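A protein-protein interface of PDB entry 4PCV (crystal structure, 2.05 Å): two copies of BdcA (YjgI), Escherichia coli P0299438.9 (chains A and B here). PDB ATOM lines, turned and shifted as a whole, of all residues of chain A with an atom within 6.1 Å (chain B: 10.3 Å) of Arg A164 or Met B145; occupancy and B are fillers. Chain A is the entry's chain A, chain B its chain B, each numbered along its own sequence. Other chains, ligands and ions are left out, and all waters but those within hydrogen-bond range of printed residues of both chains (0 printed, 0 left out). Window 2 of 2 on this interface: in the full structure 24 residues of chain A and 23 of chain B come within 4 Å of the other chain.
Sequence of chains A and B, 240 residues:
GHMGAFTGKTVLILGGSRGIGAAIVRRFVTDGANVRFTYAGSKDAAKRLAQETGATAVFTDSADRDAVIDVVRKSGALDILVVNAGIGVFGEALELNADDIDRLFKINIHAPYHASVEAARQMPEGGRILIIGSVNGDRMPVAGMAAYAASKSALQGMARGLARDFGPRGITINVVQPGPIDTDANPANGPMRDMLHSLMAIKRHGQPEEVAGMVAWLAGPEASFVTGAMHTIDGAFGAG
The guanidinium group (NH2) of Arg A160 lies within hydrogen-bond range of the side-chain hydroxyl (OG) of Ser B153.
OD2 of Asp A165 sits at hydrogen-bond distance from N of Ala B146 (3.1 Å).
N of Met B145 lies within hydrogen-bond range of OD2 of Asp A165 (3.2 Å).
The backbone carbonyl oxygen of Ala B149 sits at hydrogen-bond distance from the side-chain hydroxyl of Ser B153 (3.2 Å).
OD1 of Asp A165 is in salt-bridge range of NH1 of Arg A164.
Among the printed residues, pairs that only touch across the chains: Gly A157 with Ala B149, Gly A157 with Ser B153, Leu A162 with Ala B146, Gly A161 with Met B145, Asp A165 with Gly B144, Gly A161 with Ala B146, Arg A164 with Met B145 and Gly A157 with Ala B150.
Gly A161 touches just these residues of chain B: Met B145 (3.6 Å) and Ala B146 (3.8 Å).
No residue of chain B comes within 4 Å of Ala A163.
Arg A164 touches one residue of chain B.
Of chain A, only Gly A161 (3.6 Å), Arg A164 (3.8 Å) and Asp A165 (3.2 Å) come within 4 Å of Met B145.
Printed residues of chain A within 4 Å of Ala B146: Gly A161, Leu A162 and Asp A165.
Printed residues of chain A within 4 Å of Ala B149: Gly A157.
Of the printed residues of chain A, Ser B153 touches Gly A157 (3.2 Å) and Arg A160 (3.1 Å).
Hydrophobic or aromatic side chains of chain B that line the printed part of chain A: Met B145, Ala B146 and Ala B149.
Of the 11 printed residues of chain A, 6 touch a printed residue of chain B.
Hydrophobic or aromatic side chains of chain A within 4 Å of the printed part of chain B: Leu A162.
Along chain A the printed residues that touch a printed residue of chain B span positions 157 to 165.
No position is printed for both chains.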
ATOM      1  N   GLY A 157     -19.790 -24.586   7.819  1.00  0.00           N
ATOM      2  CA  GLY A 157     -20.471 -24.547   9.101  1.00  0.00           C
ATOM      3  C   GLY A 157     -21.916 -24.107   8.958  1.00  0.00           C
ATOM      4  O   GLY A 157     -22.808 -24.652   9.611  1.00  0.00           O
ATOM      5  N   ALA A 159     -23.865 -24.446   6.353  1.00  0.00           N
ATOM      6  CA  ALA A 159     -24.621 -25.522   5.724  1.00  0.00           C
ATOM      7  C   ALA A 159     -25.135 -26.509   6.768  1.00  0.00           C
ATOM      8  O   ALA A 159     -26.306 -26.886   6.749  1.00  0.00           O
ATOM      9  CB  ALA A 159     -23.762 -26.241   4.688  1.00  0.00           C
ATOM     10  N   ARG A 160     -24.252 -26.918   7.676  1.00  0.00           N
ATOM     11  CA  ARG A 160     -24.626 -27.812   8.768  1.00  0.00           C
ATOM     12  C   ARG A 160     -25.703 -27.195   9.652  1.00  0.00           C
ATOM     13  O   ARG A 160     -26.684 -27.851   9.996  1.00  0.00           O
ATOM     14  CB  ARG A 160     -23.405 -28.165   9.624  1.00  0.00           C
ATOM     15  CG  ARG A 160     -22.447 -29.150   8.982  1.00  0.00           C
ATOM     16  CD  ARG A 160     -21.389 -29.615   9.975  1.00  0.00           C
ATOM     17  NE  ARG A 160     -20.444 -28.557  10.324  1.00  0.00           N
ATOM     18  CZ  ARG A 160     -19.266 -28.381   9.733  1.00  0.00           C
ATOM     19  NH1 ARG A 160     -18.884 -29.191   8.757  1.00  0.00           N
ATOM     20  NH2 ARG A 160     -18.467 -27.395  10.116  1.00  0.00           N
ATOM     21  N   GLY A 161     -25.511 -25.932  10.020  1.00  0.00           N
ATOM     22  CA  GLY A 161     -26.440 -25.237  10.893  1.00  0.00           C
ATOM     23  C   GLY A 161     -27.819 -25.036  10.291  1.00  0.00           C
ATOM     24  O   GLY A 161     -28.831 -25.254  10.957  1.00  0.00           O
ATOM     25  N   LEU A 162     -27.855 -24.613   9.032  1.00  0.00           N
ATOM     26  CA  LEU A 162     -29.114 -24.395   8.325  1.00  0.00           C
ATOM     27  C   LEU A 162     -29.897 -25.693   8.154  1.00  0.00           C
ATOM     28  O   LEU A 162     -31.122 -25.711   8.288  1.00  0.00           O
ATOM     29  CB  LEU A 162     -28.860 -23.758   6.957  1.00  0.00           C
ATOM     30  CG  LEU A 162     -28.482 -22.274   6.929  1.00  0.00           C
ATOM     31  CD1 LEU A 162     -28.112 -21.845   5.518  1.00  0.00           C
ATOM     32  CD2 LEU A 162     -29.625 -21.429   7.458  1.00  0.00           C
ATOM     33  N   ALA A 163     -29.184 -26.774   7.850  1.00  0.00           N
ATOM     34  CA  ALA A 163     -29.815 -28.077   7.641  1.00  0.00           C
ATOM     35  C   ALA A 163     -30.535 -28.540   8.897  1.00  0.00           C
ATOM     36  O   ALA A 163     -31.638 -29.078   8.830  1.00  0.00           O
ATOM     37  CB  ALA A 163     -28.787 -29.101   7.219  1.00  0.00           C
ATOM     38  N   ARG A 164     -29.898 -28.330  10.043  1.00  0.00           N
ATOM     39  CA  ARG A 164     -30.514 -28.639  11.324  1.00  0.00           C
ATOM     40  C   ARG A 164     -31.751 -27.771  11.537  1.00  0.00           C
ATOM     41  O   ARG A 164     -32.791 -28.251  11.993  1.00  0.00           O
ATOM     42  CB  ARG A 164     -29.505 -28.438  12.460  1.00  0.00           C
ATOM     43  CG  ARG A 164     -30.065 -28.624  13.862  1.00  0.00           C
ATOM     44  CD  ARG A 164     -30.381 -27.284  14.516  1.00  0.00           C
ATOM     45  NE  ARG A 164     -30.703 -27.423  15.933  1.00  0.00           N
ATOM     46  CZ  ARG A 164     -31.145 -26.429  16.696  1.00  0.00           C
ATOM     47  NH1 ARG A 164     -31.325 -25.223  16.177  1.00  0.00           N
ATOM     48  NH2 ARG A 164     -31.413 -26.645  17.977  1.00  0.00           N
ATOM     49  N   ASP A 165     -31.630 -26.493  11.192  1.00  0.00           N
ATOM     50  CA  ASP A 165     -32.697 -25.523  11.417  1.00  0.00           C
ATOM     51  C   ASP A 165     -33.925 -25.762  10.539  1.00  0.00           C
ATOM     52  O   ASP A 165     -35.056 -25.666  11.013  1.00  0.00           O
ATOM     53  CB  ASP A 165     -32.177 -24.098  11.187  1.00  0.00           C
ATOM     54  CG  ASP A 165     -31.193 -23.653  12.254  1.00  0.00           C
ATOM     55  OD1 ASP A 165     -31.230 -24.210  13.370  1.00  0.00           O
ATOM     56  OD2 ASP A 165     -30.383 -22.742  11.978  1.00  0.00           O
ATOM     57  N   PHE A 166     -33.706 -26.072   9.264  1.00  0.00           N
ATOM     58  CA  PHE A 166     -34.815 -26.144   8.315  1.00  0.00           C
ATOM     59  C   PHE A 166     -35.071 -27.552   7.781  1.00  0.00           C
ATOM     60  O   PHE A 166     -35.957 -27.755   6.950  1.00  0.00           O
ATOM     61  CB  PHE A 166     -34.570 -25.181   7.154  1.00  0.00           C
ATOM     62  CG  PHE A 166     -34.473 -23.743   7.577  1.00  0.00           C
ATOM     63  CD1 PHE A 166     -35.577 -23.085   8.094  1.00  0.00           C
ATOM     64  CD2 PHE A 166     -33.282 -23.049   7.456  1.00  0.00           C
ATOM     65  CE1 PHE A 166     -35.495 -21.761   8.487  1.00  0.00           C
ATOM     66  CE2 PHE A 166     -33.192 -21.723   7.846  1.00  0.00           C
ATOM     67  CZ  PHE A 166     -34.300 -21.080   8.362  1.00  0.00           C
ATOM     68  N   GLY A 167     -34.293 -28.517   8.260  1.00  0.00           N
ATOM     69  CA  GLY A 167     -34.536 -29.922   7.972  1.00  0.00           C
ATOM     70  C   GLY A 167     -35.949 -30.395   8.284  1.00  0.00           C
ATOM     71  O   GLY A 167     -36.590 -31.014   7.433  1.00  0.00           O
ATOM     72  N   PRO A 168     -36.444 -30.117   9.506  1.00  0.00           N
ATOM     73  CA  PRO A 168     -37.831 -30.451   9.860  1.00  0.00           C
ATOM     74  C   PRO A 168     -38.882 -29.851   8.924  1.00  0.00           C
ATOM     75  O   PRO A 168     -40.023 -30.311   8.921  1.00  0.00           O
ATOM     76  CB  PRO A 168     -37.973 -29.867  11.268  1.00  0.00           C
ATOM     77  CG  PRO A 168     -36.609 -29.955  11.835  1.00  0.00           C
ATOM     78  CD  PRO A 168     -35.669 -29.696  10.689  1.00  0.00           C
ATOM     79  N   ALA B  93     -31.714 -15.905  22.349  1.00  0.00           N
ATOM     80  CA  ALA B  93     -32.832 -15.107  21.859  1.00  0.00           C
ATOM     81  C   ALA B  93     -33.791 -15.950  21.025  1.00  0.00           C
ATOM     82  O   ALA B  93     -33.387 -16.930  20.399  1.00  0.00           O
ATOM     83  CB  ALA B  93     -32.324 -13.928  21.049  1.00  0.00           C
ATOM     84  N   LEU B  94     -35.062 -15.560  21.018  1.00  0.00           N
ATOM     85  CA  LEU B  94     -36.073 -16.263  20.237  1.00  0.00           C
ATOM     86  C   LEU B  94     -35.941 -15.948  18.752  1.00  0.00           C
ATOM     87  O   LEU B  94     -36.015 -16.839  17.905  1.00  0.00           O
ATOM     88  CB  LEU B  94     -37.475 -15.897  20.725  1.00  0.00           C
ATOM     89  CG  LEU B  94     -38.642 -16.528  19.962  1.00  0.00           C
ATOM     90  CD1 LEU B  94     -38.658 -18.038  20.152  1.00  0.00           C
ATOM     91  CD2 LEU B  94     -39.964 -15.913  20.395  1.00  0.00           C
ATOM     92  N   LEU B  96     -33.715 -13.164  15.989  1.00  0.00           N
ATOM     93  CA  LEU B  96     -32.695 -12.144  15.779  1.00  0.00           C
ATOM     94  C   LEU B  96     -32.992 -11.344  14.516  1.00  0.00           C
ATOM     95  O   LEU B  96     -33.279 -11.923  13.468  1.00  0.00           O
ATOM     96  CB  LEU B  96     -31.313 -12.794  15.682  1.00  0.00           C
ATOM     97  CG  LEU B  96     -30.257 -12.426  16.725  1.00  0.00           C
ATOM     98  CD1 LEU B  96     -30.860 -12.361  18.115  1.00  0.00           C
ATOM     99  CD2 LEU B  96     -29.117 -13.432  16.686  1.00  0.00           C
ATOM    100  N   ILE B 101     -27.837 -10.003  13.570  1.00  0.00           N
ATOM    101  CA  ILE B 101     -27.146 -11.092  12.888  1.00  0.00           C
ATOM    102  C   ILE B 101     -25.818 -10.596  12.325  1.00  0.00           C
ATOM    103  O   ILE B 101     -24.777 -11.224  12.521  1.00  0.00           O
ATOM    104  CB  ILE B 101     -28.002 -11.684  11.749  1.00  0.00           C
ATOM    105  CG1 ILE B 101     -29.132 -12.542  12.319  1.00  0.00           C
ATOM    106  CG2 ILE B 101     -27.139 -12.516  10.801  1.00  0.00           C
ATOM    107  CD1 ILE B 101     -28.652 -13.784  13.040  1.00  0.00           C
ATOM    108  N   LEU B 104     -23.474 -10.085  15.077  1.00  0.00           N
ATOM    109  CA  LEU B 104     -22.930 -11.373  15.497  1.00  0.00           C
ATOM    110  C   LEU B 104     -21.732 -11.755  14.631  1.00  0.00           C
ATOM    111  O   LEU B 104     -20.668 -12.104  15.143  1.00  0.00           O
ATOM    112  CB  LEU B 104     -24.016 -12.455  15.429  1.00  0.00           C
ATOM    113  CG  LEU B 104     -23.737 -13.867  15.954  1.00  0.00           C
ATOM    114  CD1 LEU B 104     -25.041 -14.515  16.383  1.00  0.00           C
ATOM    115  CD2 LEU B 104     -23.048 -14.739  14.913  1.00  0.00           C
ATOM    116  N   PHE B 105     -21.918 -11.684  13.316  1.00  0.00           N
ATOM    117  CA  PHE B 105     -20.862 -12.016  12.367  1.00  0.00           C
ATOM    118  C   PHE B 105     -19.658 -11.086  12.508  1.00  0.00           C
ATOM    119  O   PHE B 105     -18.515 -11.528  12.433  1.00  0.00           O
ATOM    120  CB  PHE B 105     -21.401 -11.964  10.932  1.00  0.00           C
ATOM    121  CG  PHE B 105     -22.279 -13.132  10.573  1.00  0.00           C
ATOM    122  CD1 PHE B 105     -22.052 -14.384  11.127  1.00  0.00           C
ATOM    123  CD2 PHE B 105     -23.331 -12.979   9.680  1.00  0.00           C
ATOM    124  CE1 PHE B 105     -22.856 -15.460  10.798  1.00  0.00           C
ATOM    125  CE2 PHE B 105     -24.137 -14.051   9.346  1.00  0.00           C
ATOM    126  CZ  PHE B 105     -23.901 -15.294   9.906  1.00  0.00           C
ATOM    127  N   ASN B 108     -17.940 -12.087  15.832  1.00  0.00           N
ATOM    128  CA  ASN B 108     -17.383 -13.438  15.841  1.00  0.00           C
ATOM    129  C   ASN B 108     -16.447 -13.752  14.675  1.00  0.00           C
ATOM    130  O   ASN B 108     -15.643 -14.679  14.760  1.00  0.00           O
ATOM    131  CB  ASN B 108     -18.514 -14.466  15.870  1.00  0.00           C
ATOM    132  CG  ASN B 108     -19.151 -14.590  17.241  1.00  0.00           C
ATOM    133  OD1 ASN B 108     -19.945 -13.743  17.652  1.00  0.00           O
ATOM    134  ND2 ASN B 108     -18.806 -15.653  17.957  1.00  0.00           N
ATOM    135  N   SER B 134     -17.402 -18.599  21.255  1.00  0.00           N
ATOM    136  CA  SER B 134     -18.644 -18.385  21.984  1.00  0.00           C
ATOM    137  C   SER B 134     -18.919 -19.530  22.952  1.00  0.00           C
ATOM    138  O   SER B 134     -18.637 -20.688  22.648  1.00  0.00           O
ATOM    139  CB  SER B 134     -19.815 -18.233  21.009  1.00  0.00           C
ATOM    140  OG  SER B 134     -19.502 -17.326  19.967  1.00  0.00           O
ATOM    141  N   VAL B 135     -19.465 -19.202  24.119  1.00  0.00           N
ATOM    142  CA  VAL B 135     -19.831 -20.220  25.098  1.00  0.00           C
ATOM    143  C   VAL B 135     -21.092 -20.961  24.665  1.00  0.00           C
ATOM    144  O   VAL B 135     -22.078 -20.347  24.257  1.00  0.00           O
ATOM    145  CB  VAL B 135     -20.050 -19.613  26.498  1.00  0.00           C
ATOM    146  CG1 VAL B 135     -18.718 -19.377  27.188  1.00  0.00           C
ATOM    147  CG2 VAL B 135     -20.848 -18.322  26.405  1.00  0.00           C
ATOM    148  N   ASN B 136     -21.049 -22.287  24.749  1.00  0.00           N
ATOM    149  CA  ASN B 136     -22.180 -23.117  24.353  1.00  0.00           C
ATOM    150  C   ASN B 136     -23.086 -23.444  25.535  1.00  0.00           C
ATOM    151  O   ASN B 136     -23.456 -22.560  26.307  1.00  0.00           O
ATOM    152  CB  ASN B 136     -21.688 -24.408  23.697  1.00  0.00           C
ATOM    153  N   GLY B 144     -32.099 -21.003  16.438  1.00  0.00           N
ATOM    154  CA  GLY B 144     -31.281 -21.015  15.239  1.00  0.00           C
ATOM    155  C   GLY B 144     -29.816 -21.264  15.546  1.00  0.00           C
ATOM    156  O   GLY B 144     -29.216 -20.569  16.365  1.00  0.00           O
ATOM    157  N   MET B 145     -29.237 -22.257  14.881  1.00  0.00           N
ATOM    158  CA  MET B 145     -27.852 -22.635  15.131  1.00  0.00           C
ATOM    159  C   MET B 145     -26.933 -22.165  14.005  1.00  0.00           C
ATOM    160  O   MET B 145     -25.714 -22.105  14.173  1.00  0.00           O
ATOM    161  CB  MET B 145     -27.739 -24.152  15.300  1.00  0.00           C
ATOM    162  CG  MET B 145     -26.483 -24.607  16.022  1.00  0.00           C
ATOM    163  SD  MET B 145     -26.254 -26.392  15.953  1.00  0.00           S
ATOM    164  CE  MET B 145     -25.948 -26.620  14.206  1.00  0.00           C
ATOM    165  N   ALA B 146     -27.532 -21.823  12.867  1.00  0.00           N
ATOM    166  CA  ALA B 146     -26.792 -21.534  11.638  1.00  0.00           C
ATOM    167  C   ALA B 146     -25.731 -20.446  11.793  1.00  0.00           C
ATOM    168  O   ALA B 146     -24.598 -20.610  11.337  1.00  0.00           O
ATOM    169  CB  ALA B 146     -27.765 -21.151  10.531  1.00  0.00           C
ATOM    170  N   ALA B 147     -26.095 -19.337  12.428  1.00  0.00           N
ATOM    171  CA  ALA B 147     -25.161 -18.227  12.603  1.00  0.00           C
ATOM    172  C   ALA B 147     -24.001 -18.617  13.517  1.00  0.00           C
ATOM    173  O   ALA B 147     -22.852 -18.250  13.273  1.00  0.00           O
ATOM    174  CB  ALA B 147     -25.884 -17.005  13.154  1.00  0.00           C
ATOM    175  N   TYR B 148     -24.317 -19.358  14.573  1.00  0.00           N
ATOM    176  CA  TYR B 148     -23.308 -19.839  15.508  1.00  0.00           C
ATOM    177  C   TYR B 148     -22.372 -20.849  14.848  1.00  0.00           C
ATOM    178  O   TYR B 148     -21.158 -20.809  15.048  1.00  0.00           O
ATOM    179  CB  TYR B 148     -23.981 -20.464  16.734  1.00  0.00           C
ATOM    180  CG  TYR B 148     -23.074 -21.356  17.554  1.00  0.00           C
ATOM    181  CD1 TYR B 148     -22.152 -20.817  18.442  1.00  0.00           C
ATOM    182  CD2 TYR B 148     -23.147 -22.741  17.445  1.00  0.00           C
ATOM    183  CE1 TYR B 148     -21.324 -21.630  19.193  1.00  0.00           C
ATOM    184  CE2 TYR B 148     -22.324 -23.561  18.192  1.00  0.00           C
ATOM    185  CZ  TYR B 148     -21.415 -22.999  19.064  1.00  0.00           C
ATOM    186  OH  TYR B 148     -20.595 -23.812  19.810  1.00  0.00           O
ATOM    187  N   ALA B 149     -22.949 -21.753  14.064  1.00  0.00           N
ATOM    188  CA  ALA B 149     -22.175 -22.783  13.379  1.00  0.00           C
ATOM    189  C   ALA B 149     -21.205 -22.170  12.376  1.00  0.00           C
ATOM    190  O   ALA B 149     -20.044 -22.573  12.292  1.00  0.00           O
ATOM    191  CB  ALA B 149     -23.104 -23.762  12.684  1.00  0.00           C
ATOM    192  N   ALA B 150     -21.687 -21.189  11.622  1.00  0.00           N
ATOM    193  CA  ALA B 150     -20.868 -20.508  10.627  1.00  0.00           C
ATOM    194  C   ALA B 150     -19.696 -19.775  11.277  1.00  0.00           C
ATOM    195  O   ALA B 150     -18.571 -19.836  10.787  1.00  0.00           O
ATOM    196  CB  ALA B 150     -21.717 -19.538   9.821  1.00  0.00           C
ATOM    197  N   SER B 151     -19.970 -19.085  12.380  1.00  0.00           N
ATOM    198  CA  SER B 151     -18.948 -18.312  13.082  1.00  0.00           C
ATOM    199  C   SER B 151     -17.858 -19.201  13.677  1.00  0.00           C
ATOM    200  O   SER B 151     -16.671 -18.899  13.564  1.00  0.00           O
ATOM    201  CB  SER B 151     -19.588 -17.464  14.182  1.00  0.00           C
ATOM    202  OG  SER B 151     -20.476 -16.506  13.632  1.00  0.00           O
ATOM    203  N   LYS B 152     -18.266 -20.296  14.313  1.00  0.00           N
ATOM    204  CA  LYS B 152     -17.314 -21.230  14.909  1.00  0.00           C
ATOM    205  C   LYS B 152     -16.404 -21.852  13.852  1.00  0.00           C
ATOM    206  O   LYS B 152     -15.190 -21.961  14.045  1.00  0.00           O
ATOM    207  CB  LYS B 152     -18.051 -22.328  15.676  1.00  0.00           C
ATOM    208  CG  LYS B 152     -17.130 -23.380  16.272  1.00  0.00           C
ATOM    209  CD  LYS B 152     -17.909 -24.422  17.056  1.00  0.00           C
ATOM    210  CE  LYS B 152     -16.976 -25.460  17.660  1.00  0.00           C
ATOM    211  NZ  LYS B 152     -17.701 -26.427  18.529  1.00  0.00           N
ATOM    212  N   SER B 153     -16.995 -22.263  12.735  1.00  0.00           N
ATOM    213  CA  SER B 153     -16.228 -22.848  11.641  1.00  0.00           C
ATOM    214  C   SER B 153     -15.293 -21.818  11.025  1.00  0.00           C
ATOM    215  O   SER B 153     -14.154 -22.131  10.680  1.00  0.00           O
ATOM    216  CB  SER B 153     -17.159 -23.420  10.568  1.00  0.00           C
ATOM    217  OG  SER B 153     -17.894 -24.525  11.060  1.00  0.00           O
